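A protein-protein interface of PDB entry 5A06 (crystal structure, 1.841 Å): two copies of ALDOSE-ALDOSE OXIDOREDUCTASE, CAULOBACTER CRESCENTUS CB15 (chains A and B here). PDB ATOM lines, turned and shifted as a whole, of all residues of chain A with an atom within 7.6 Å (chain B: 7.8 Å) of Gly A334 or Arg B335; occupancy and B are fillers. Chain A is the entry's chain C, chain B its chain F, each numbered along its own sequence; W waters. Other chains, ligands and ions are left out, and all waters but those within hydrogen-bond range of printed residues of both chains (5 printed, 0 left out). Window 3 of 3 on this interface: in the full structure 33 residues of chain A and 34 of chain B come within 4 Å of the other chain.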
ATOM      1  N   ASN A 206      24.868 -18.696  22.595  1.00  0.00           N
ATOM      2  CA  ASN A 206      25.756 -17.715  21.959  1.00  0.00           C
ATOM      3  C   ASN A 206      26.469 -18.346  20.771  1.00  0.00           C
ATOM      4  O   ASN A 206      26.685 -19.555  20.766  1.00  0.00           O
ATOM      5  CB  ASN A 206      26.834 -17.208  22.924  1.00  0.00           C
ATOM      6  CG  ASN A 206      26.368 -16.065  23.794  1.00  0.00           C
ATOM      7  OD1 ASN A 206      25.429 -15.338  23.459  1.00  0.00           O
ATOM      8  ND2 ASN A 206      27.039 -15.895  24.930  1.00  0.00           N
ATOM      9  N   ALA A 207      26.881 -17.545  19.791  1.00  0.00           N
ATOM     10  CA  ALA A 207      27.698 -18.069  18.701  1.00  0.00           C
ATOM     11  C   ALA A 207      28.523 -16.999  17.989  1.00  0.00           C
ATOM     12  O   ALA A 207      28.158 -15.831  17.958  1.00  0.00           O
ATOM     13  CB  ALA A 207      26.823 -18.818  17.680  1.00  0.00           C
ATOM     14  N   TYR A 328      22.727 -20.322  14.452  1.00  0.00           N
ATOM     15  CA  TYR A 328      22.869 -19.466  13.291  1.00  0.00           C
ATOM     16  C   TYR A 328      22.320 -18.056  13.589  1.00  0.00           C
ATOM     17  O   TYR A 328      22.923 -17.057  13.198  1.00  0.00           O
ATOM     18  CB  TYR A 328      22.150 -20.082  12.073  1.00  0.00           C
ATOM     19  CG  TYR A 328      22.907 -21.207  11.378  1.00  0.00           C
ATOM     20  CD1 TYR A 328      24.257 -21.079  11.061  1.00  0.00           C
ATOM     21  CD2 TYR A 328      22.251 -22.381  11.001  1.00  0.00           C
ATOM     22  CE1 TYR A 328      24.940 -22.103  10.399  1.00  0.00           C
ATOM     23  CE2 TYR A 328      22.916 -23.405  10.346  1.00  0.00           C
ATOM     24  CZ  TYR A 328      24.258 -23.266  10.053  1.00  0.00           C
ATOM     25  OH  TYR A 328      24.907 -24.286   9.401  1.00  0.00           O
ATOM     26  N   ARG A 329      21.193 -17.971  14.285  1.00  0.00           N
ATOM     27  CA  ARG A 329      20.617 -16.659  14.600  1.00  0.00           C
ATOM     28  C   ARG A 329      21.538 -15.857  15.533  1.00  0.00           C
ATOM     29  O   ARG A 329      21.740 -14.654  15.338  1.00  0.00           O
ATOM     30  CB  ARG A 329      19.221 -16.819  15.225  1.00  0.00           C
ATOM     31  CG  ARG A 329      18.511 -15.497  15.567  1.00  0.00           C
ATOM     32  CD  ARG A 329      17.114 -15.747  16.170  1.00  0.00           C
ATOM     33  NE  ARG A 329      16.308 -16.622  15.317  1.00  0.00           N
ATOM     34  CZ  ARG A 329      15.892 -17.849  15.645  1.00  0.00           C
ATOM     35  NH1 ARG A 329      16.179 -18.376  16.838  1.00  0.00           N
ATOM     36  NH2 ARG A 329      15.174 -18.558  14.775  1.00  0.00           N
ATOM     37  N   ALA A 330      22.121 -16.535  16.520  1.00  0.00           N
ATOM     38  CA  ALA A 330      22.974 -15.872  17.515  1.00  0.00           C
ATOM     39  C   ALA A 330      24.220 -15.284  16.867  1.00  0.00           C
ATOM     40  O   ALA A 330      24.680 -14.200  17.238  1.00  0.00           O
ATOM     41  CB  ALA A 330      23.364 -16.854  18.608  1.00  0.00           C
ATOM     42  N   ALA A 331      24.775 -16.011  15.908  1.00  0.00           N
ATOM     43  CA  ALA A 331      25.961 -15.552  15.194  1.00  0.00           C
ATOM     44  C   ALA A 331      25.601 -14.377  14.295  1.00  0.00           C
ATOM     45  O   ALA A 331      26.351 -13.412  14.172  1.00  0.00           O
ATOM     46  CB  ALA A 331      26.570 -16.696  14.363  1.00  0.00           C
ATOM     47  N   ARG A 332      24.440 -14.475  13.666  1.00  0.00           N
ATOM     48  CA  ARG A 332      23.951 -13.447  12.751  1.00  0.00           C
ATOM     49  C   ARG A 332      23.641 -12.128  13.477  1.00  0.00           C
ATOM     50  O   ARG A 332      24.038 -11.048  13.026  1.00  0.00           O
ATOM     51  CB  ARG A 332      22.709 -13.982  12.032  1.00  0.00           C
ATOM     52  CG  ARG A 332      22.214 -13.177  10.856  1.00  0.00           C
ATOM     53  CD  ARG A 332      21.208 -14.002  10.045  1.00  0.00           C
ATOM     54  NE  ARG A 332      20.013 -14.356  10.816  1.00  0.00           N
ATOM     55  CZ  ARG A 332      19.599 -15.602  11.053  1.00  0.00           C
ATOM     56  NH1 ARG A 332      20.275 -16.644  10.584  1.00  0.00           N
ATOM     57  NH2 ARG A 332      18.497 -15.806  11.765  1.00  0.00           N
ATOM     58  N   GLU A 333      22.941 -12.215  14.602  1.00  0.00           N
ATOM     59  CA  GLU A 333      22.489 -11.033  15.321  1.00  0.00           C
ATOM     60  C   GLU A 333      23.446 -10.557  16.419  1.00  0.00           C
ATOM     61  O   GLU A 333      23.269  -9.471  16.966  1.00  0.00           O
ATOM     62  CB  GLU A 333      21.110 -11.296  15.937  1.00  0.00           C
ATOM     63  CG  GLU A 333      20.028 -11.539  14.890  1.00  0.00           C
ATOM     64  CD  GLU A 333      18.668 -11.845  15.486  1.00  0.00           C
ATOM     65  OE1 GLU A 333      18.527 -11.806  16.725  1.00  0.00           O
ATOM     66  OE2 GLU A 333      17.737 -12.135  14.707  1.00  0.00           O
ATOM     67  N   GLY A 334      24.454 -11.354  16.756  1.00  0.00           N
ATOM     68  CA  GLY A 334      25.367 -10.935  17.808  1.00  0.00           C
ATOM     69  C   GLY A 334      24.695 -10.795  19.164  1.00  0.00           C
ATOM     70  O   GLY A 334      24.938  -9.838  19.919  1.00  0.00           O
ATOM     71  N   ARG A 335      23.847 -11.761  19.496  1.00  0.00           N
ATOM     72  CA  ARG A 335      23.185 -11.731  20.781  1.00  0.00           C
ATOM     73  C   ARG A 335      22.897 -13.136  21.303  1.00  0.00           C
ATOM     74  O   ARG A 335      22.932 -14.128  20.557  1.00  0.00           O
ATOM     75  CB  ARG A 335      21.886 -10.919  20.697  1.00  0.00           C
ATOM     76  CG  ARG A 335      20.858 -11.516  19.779  1.00  0.00           C
ATOM     77  CD  ARG A 335      19.507 -10.797  19.878  1.00  0.00           C
ATOM     78  NE  ARG A 335      18.495 -11.503  19.091  1.00  0.00           N
ATOM     79  CZ  ARG A 335      17.683 -12.446  19.571  1.00  0.00           C
ATOM     80  NH1 ARG A 335      17.739 -12.792  20.855  1.00  0.00           N
ATOM     81  NH2 ARG A 335      16.807 -13.038  18.763  1.00  0.00           N
ATOM     82  N   THR A 336      22.644 -13.214  22.599  1.00  0.00           N
ATOM     83  CA  THR A 336      22.249 -14.462  23.229  1.00  0.00           C
ATOM     84  C   THR A 336      20.812 -14.769  22.844  1.00  0.00           C
ATOM     85  O   THR A 336      19.936 -13.936  23.037  1.00  0.00           O
ATOM     86  CB  THR A 336      22.376 -14.384  24.756  1.00  0.00           C
ATOM     87  OG1 THR A 336      23.718 -14.020  25.088  1.00  0.00           O
ATOM     88  CG2 THR A 336      22.055 -15.733  25.386  1.00  0.00           C
ATOM     89  N   VAL A 337      20.586 -15.949  22.268  1.00  0.00           N
ATOM     90  CA  VAL A 337      19.257 -16.351  21.830  1.00  0.00           C
ATOM     91  C   VAL A 337      18.652 -17.278  22.872  1.00  0.00           C
ATOM     92  O   VAL A 337      19.283 -18.252  23.290  1.00  0.00           O
ATOM     93  CB  VAL A 337      19.306 -17.035  20.431  1.00  0.00           C
ATOM     94  CG1 VAL A 337      17.967 -17.668  20.073  1.00  0.00           C
ATOM     95  CG2 VAL A 337      19.728 -16.036  19.371  1.00  0.00           C
ATOM     96  N   VAL B 205      33.526 -10.249  21.622  1.00  0.00           N
ATOM     97  CA  VAL B 205      33.459 -11.120  22.791  1.00  0.00           C
ATOM     98  C   VAL B 205      32.016 -11.533  23.092  1.00  0.00           C
ATOM     99  O   VAL B 205      31.120 -10.673  23.196  1.00  0.00           O
ATOM    100  CB  VAL B 205      34.035 -10.417  24.044  1.00  0.00           C
ATOM    101  CG1 VAL B 205      34.075 -11.371  25.229  1.00  0.00           C
ATOM    102  CG2 VAL B 205      35.418  -9.833  23.769  1.00  0.00           C
ATOM    103  N   ASN B 206      31.805 -12.846  23.221  1.00  0.00           N
ATOM    104  CA  ASN B 206      30.585 -13.428  23.797  1.00  0.00           C
ATOM    105  C   ASN B 206      30.886 -14.017  25.171  1.00  0.00           C
ATOM    106  O   ASN B 206      32.004 -14.473  25.408  1.00  0.00           O
ATOM    107  CB  ASN B 206      30.029 -14.559  22.922  1.00  0.00           C
ATOM    108  CG  ASN B 206      29.163 -14.062  21.789  1.00  0.00           C
ATOM    109  OD1 ASN B 206      28.639 -12.942  21.822  1.00  0.00           O
ATOM    110  ND2 ASN B 206      29.008 -14.897  20.773  1.00  0.00           N
ATOM    111  N   ALA B 207      29.896 -14.075  26.050  1.00  0.00           N
ATOM    112  CA  ALA B 207      30.101 -14.779  27.326  1.00  0.00           C
ATOM    113  C   ALA B 207      28.811 -15.327  27.922  1.00  0.00           C
ATOM    114  O   ALA B 207      27.722 -14.804  27.672  1.00  0.00           O
ATOM    115  CB  ALA B 207      30.796 -13.861  28.358  1.00  0.00           C
ATOM    116  N   ALA B 326      34.951  -6.456  29.091  1.00  0.00           N
ATOM    117  CA  ALA B 326      34.052  -6.801  27.980  1.00  0.00           C
ATOM    118  C   ALA B 326      33.342  -8.137  28.226  1.00  0.00           C
ATOM    119  O   ALA B 326      32.154  -8.294  27.922  1.00  0.00           O
ATOM    120  CB  ALA B 326      34.831  -6.849  26.657  1.00  0.00           C
ATOM    121  N   ILE B 327      34.071  -9.097  28.802  1.00  0.00           N
ATOM    122  CA  ILE B 327      33.514 -10.423  29.081  1.00  0.00           C
ATOM    123  C   ILE B 327      32.382 -10.338  30.116  1.00  0.00           C
ATOM    124  O   ILE B 327      31.315 -10.927  29.929  1.00  0.00           O
ATOM    125  CB  ILE B 327      34.630 -11.420  29.581  1.00  0.00           C
ATOM    126  CG1 ILE B 327      35.577 -11.801  28.427  1.00  0.00           C
ATOM    127  CG2 ILE B 327      33.997 -12.669  30.191  1.00  0.00           C
ATOM    128  CD1 ILE B 327      36.923 -12.407  28.907  1.00  0.00           C
ATOM    129  N   ARG B 329      30.618  -7.748  30.756  1.00  0.00           N
ATOM    130  CA  ARG B 329      29.536  -7.000  30.123  1.00  0.00           C
ATOM    131  C   ARG B 329      28.714  -7.868  29.160  1.00  0.00           C
ATOM    132  O   ARG B 329      27.477  -7.773  29.132  1.00  0.00           O
ATOM    133  CB  ARG B 329      30.098  -5.793  29.390  1.00  0.00           C
ATOM    134  CG  ARG B 329      29.024  -4.872  28.793  1.00  0.00           C
ATOM    135  CD  ARG B 329      29.707  -3.738  28.048  1.00  0.00           C
ATOM    136  NE  ARG B 329      28.788  -2.668  27.690  1.00  0.00           N
ATOM    137  CZ  ARG B 329      28.954  -1.857  26.646  1.00  0.00           C
ATOM    138  NH1 ARG B 329      29.993  -2.014  25.828  1.00  0.00           N
ATOM    139  NH2 ARG B 329      28.061  -0.902  26.399  1.00  0.00           N
ATOM    140  N   ALA B 330      29.394  -8.702  28.374  1.00  0.00           N
ATOM    141  CA  ALA B 330      28.717  -9.581  27.413  1.00  0.00           C
ATOM    142  C   ALA B 330      27.819 -10.569  28.134  1.00  0.00           C
ATOM    143  O   ALA B 330      26.716 -10.871  27.678  1.00  0.00           O
ATOM    144  CB  ALA B 330      29.742 -10.328  26.529  1.00  0.00           C
ATOM    145  N   ALA B 331      28.291 -11.085  29.269  1.00  0.00           N
ATOM    146  CA  ALA B 331      27.466 -12.010  30.042  1.00  0.00           C
ATOM    147  C   ALA B 331      26.274 -11.306  30.702  1.00  0.00           C
ATOM    148  O   ALA B 331      25.195 -11.891  30.819  1.00  0.00           O
ATOM    149  CB  ALA B 331      28.321 -12.730  31.099  1.00  0.00           C
ATOM    150  N   ARG B 332      26.469 -10.060  31.141  1.00  0.00           N
ATOM    151  CA  ARG B 332      25.405  -9.277  31.783  1.00  0.00           C
ATOM    152  C   ARG B 332      24.319  -8.870  30.775  1.00  0.00           C
ATOM    153  O   ARG B 332      23.122  -8.989  31.046  1.00  0.00           O
ATOM    154  CB  ARG B 332      25.999  -8.026  32.466  1.00  0.00           C
ATOM    155  CG  ARG B 332      24.985  -7.156  33.237  1.00  0.00           C
ATOM    156  CD  ARG B 332      25.676  -6.096  34.135  1.00  0.00           C
ATOM    157  NE  ARG B 332      26.791  -5.431  33.455  1.00  0.00           N
ATOM    158  CZ  ARG B 332      28.075  -5.574  33.800  1.00  0.00           C
ATOM    159  NH1 ARG B 332      28.411  -6.321  34.845  1.00  0.00           N
ATOM    160  NH2 ARG B 332      29.030  -4.946  33.112  1.00  0.00           N
ATOM    161  N   GLU B 333      24.739  -8.423  29.599  1.00  0.00           N
ATOM    162  CA  GLU B 333      23.793  -7.897  28.614  1.00  0.00           C
ATOM    163  C   GLU B 333      23.307  -8.941  27.609  1.00  0.00           C
ATOM    164  O   GLU B 333      22.354  -8.702  26.872  1.00  0.00           O
ATOM    165  CB  GLU B 333      24.423  -6.712  27.888  1.00  0.00           C
ATOM    166  CG  GLU B 333      24.894  -5.615  28.860  1.00  0.00           C
ATOM    167  CD  GLU B 333      25.350  -4.336  28.169  1.00  0.00           C
ATOM    168  OE1 GLU B 333      25.354  -4.285  26.920  1.00  0.00           O
ATOM    169  OE2 GLU B 333      25.710  -3.375  28.882  1.00  0.00           O
ATOM    170  N   GLY B 334      23.946 -10.100  27.577  1.00  0.00           N
ATOM    171  CA  GLY B 334      23.539 -11.146  26.647  1.00  0.00           C
ATOM    172  C   GLY B 334      23.719 -10.739  25.196  1.00  0.00           C
ATOM    173  O   GLY B 334      22.836 -10.933  24.367  1.00  0.00           O
ATOM    174  N   ARG B 335      24.864 -10.142  24.881  1.00  0.00           N
ATOM    175  CA  ARG B 335      25.134  -9.758  23.512  1.00  0.00           C
ATOM    176  C   ARG B 335      26.629  -9.778  23.242  1.00  0.00           C
ATOM    177  O   ARG B 335      27.453  -9.848  24.156  1.00  0.00           O
ATOM    178  CB  ARG B 335      24.568  -8.367  23.212  1.00  0.00           C
ATOM    179  CG  ARG B 335      25.267  -7.290  24.004  1.00  0.00           C
ATOM    180  CD  ARG B 335      24.864  -5.893  23.590  1.00  0.00           C
ATOM    181  NE  ARG B 335      25.599  -4.911  24.386  1.00  0.00           N
ATOM    182  CZ  ARG B 335      26.752  -4.354  24.015  1.00  0.00           C
ATOM    183  NH1 ARG B 335      27.304  -4.664  22.846  1.00  0.00           N
ATOM    184  NH2 ARG B 335      27.348  -3.478  24.813  1.00  0.00           N
ATOM    185  N   THR B 336      26.968  -9.726  21.971  1.00  0.00           N
ATOM    186  CA  THR B 336      28.347  -9.682  21.546  1.00  0.00           C
ATOM    187  C   THR B 336      28.861  -8.266  21.768  1.00  0.00           C
ATOM    188  O   THR B 336      28.266  -7.302  21.292  1.00  0.00           O
ATOM    189  CB  THR B 336      28.468 -10.091  20.072  1.00  0.00           C
ATOM    190  OG1 THR B 336      27.882 -11.390  19.910  1.00  0.00           O
ATOM    191  CG2 THR B 336      29.938 -10.112  19.612  1.00  0.00           C
ATOM    192  N   VAL B 337      29.944  -8.142  22.516  1.00  0.00           N
ATOM    193  CA  VAL B 337      30.525  -6.837  22.806  1.00  0.00           C
ATOM    194  C   VAL B 337      31.702  -6.595  21.863  1.00  0.00           C
ATOM    195  O   VAL B 337      32.563  -7.456  21.707  1.00  0.00           O
ATOM    196  CB  VAL B 337      30.971  -6.751  24.293  1.00  0.00           C
ATOM    197  CG1 VAL B 337      31.767  -5.457  24.565  1.00  0.00           C
ATOM    198  CG2 VAL B 337      29.757  -6.844  25.212  1.00  0.00           C
ATOM    199  N   LYS B 338      31.727  -5.431  21.214  1.00  0.00           N
ATOM    200  CA  LYS B 338      32.789  -5.131  20.258  1.00  0.00           C
ATOM    201  C   LYS B 338      33.916  -4.354  20.920  1.00  0.00           C
ATOM    202  O   LYS B 338      33.673  -3.501  21.778  1.00  0.00           O
ATOM    203  CB  LYS B 338      32.225  -4.353  19.062  1.00  0.00           C
ATOM    204  CG  LYS B 338      31.379  -5.221  18.135  1.00  0.00           C
ATOM    205  CD  LYS B 338      30.436  -4.408  17.252  1.00  0.00           C
ATOM    206  CE  LYS B 338      31.184  -3.555  16.243  1.00  0.00           C
ATOM    207  NZ  LYS B 338      30.249  -2.941  15.250  1.00  0.00           N
HETATM  208  O   HOH W   1      25.977 -12.732  22.493  1.00  0.00           O
HETATM  209  O   HOH W   2      24.887 -14.580  27.606  1.00  0.00           O
HETATM  210  O   HOH W   3      27.340 -12.775  25.351  1.00  0.00           O
HETATM  211  O   HOH W   4      28.671 -13.023  17.718  1.00  0.00           O
HETATM  212  O   HOH W   5      26.070 -14.622  19.893  1.00  0.00           O
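The backbone carbonyl oxygen (O) of Ala B330 lies within hydrogen-bond range of the backbone NH (N) of Arg B335, 3.4 Å away.
The side-chain carboxylate (OE1) of Glu A333 lies within salt-bridge range of the guanidinium group (NH2) of Arg A335 (2.9 Å).
The side-chain carboxylate of Glu B333 lies within salt-bridge range of the guanidinium group of Arg B335 (2.6 Å).
The side-chain amide oxygen of Asn B206 sits at hydrogen-bond distance from the side-chain hydroxyl of Thr B336, 2.6 Å away.
The side-chain amide oxygen of Asn A206 sits at hydrogen-bond distance from the side-chain hydroxyl of Thr A336, 2.7 Å away.
The backbone carbonyl oxygen (O) of Ala A330 lies within hydrogen-bond range of the backbone NH (N) of Arg A335.
Asn A206 touches its own counterpart, Asn B206.
Asn A206 touches Ala B207, and with the chains exchanged Ala A207 touches Asn B206.
Gly A334 touches Thr B336, and with the chains exchanged Thr A336 touches Gly B334.
Arg A335 touches its own counterpart, Arg B335.
Positions printed for both chains: 206, 207, 329, 330, 331, 332, 333, 334, 335, 336 and 337.
The side-chain amide nitrogen of Asn B206 is in hydrogen-bond range of the backbone carbonyl oxygen of Ala A207, 3.1 Å away.
The backbone NH (N) of Thr B336 is in hydrogen-bond range of the backbone carbonyl oxygen (O) of Gly A334.
O of Ala B207 lies within hydrogen-bond range of ND2 of Asn A206 (3.0 Å).
O of Gly B334 lies within hydrogen-bond range of N of Thr A336, 2.9 Å away.
Of the printed residues of chain B, Gly A334 touches Arg B335 and Thr B336.
Of chain A, only Gly A334 (3.6 Å) and Arg A335 (3.9 Å) come within 4 Å of Arg B335.
Of chain A, only Arg A335 and Thr A336 come within 4 Å of Gly B334.
Of the printed residues of chain A, Ala B207 touches Asn A206 (3.0 Å).
Of the printed residues of chain A, Thr B336 touches Gly A334 (2.9 Å).
Of the printed residues of chain B, Asn A206 touches Asn B206 (3.8 Å) and Ala B207 (3.0 Å).
Of the printed residues of chain B, Thr A336 touches Gly B334 (2.9 Å).
Printed residues of chain A within 4 Å of Asn B206: Asn A206 and Ala A207.
The nearest residue of chain B that does not touch Gly A334 is Gly B334 (5.0 Å).
The nearest printed residue of chain A that does not touch Thr B336 is Arg A335 (4.1 Å).
Of the 12 printed residues of chain A, 5 touch a printed residue of chain B.
Printed residues of chain B that touch a printed residue of chain A: Asn B206, Ala B207, Gly B334, Arg B335 and Thr B336.
Among the printed residues, 8 pairs touch across the chains.
Among the printed residues, no Asp or Glu carboxylate lies within 4 Å of a Lys or Arg side-chain nitrogen of the other chain.
Water W1 lies within hydrogen-bond range of OD1 of Asn B206 (2.8 Å), OD1 of Asn A206 (2.8 Å), N of Thr B336 (3.2 Å) and N of Thr A336 (3.4 Å).
Water W2 bridges OG1 of Thr A336 and O of Ala B207.
Water W4 bridges OG1 of Thr B336 (2.8 Å) and O of Ala A207 (2.9 Å).
Water W3 lies within hydrogen-bond range of the backbone NH (N) of Ala B207 (3.0 Å), the backbone carbonyl oxygen (O) of Ala B330 (3.1 Å), the side-chain amide nitrogen (ND2) of Asn A206 (3.2 Å) and the backbone carbonyl oxygen (O) of Arg B335 (3.2 Å).
Water W5 lies within hydrogen-bond range of the backbone carbonyl oxygen of Ala A330, the backbone NH of Ala A207, the side-chain amide nitrogen of Asn B206 and the backbone carbonyl oxygen of Arg A335.
Asn B206 touches Asn A206.
CA of Arg B335 touches O of Gly A334 (3.6 Å).
Arg A335 touches Gly B334 (CA to O, 3.7 Å).
Arg A335 touches Arg B335 (CA to CA, 3.9 Å).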
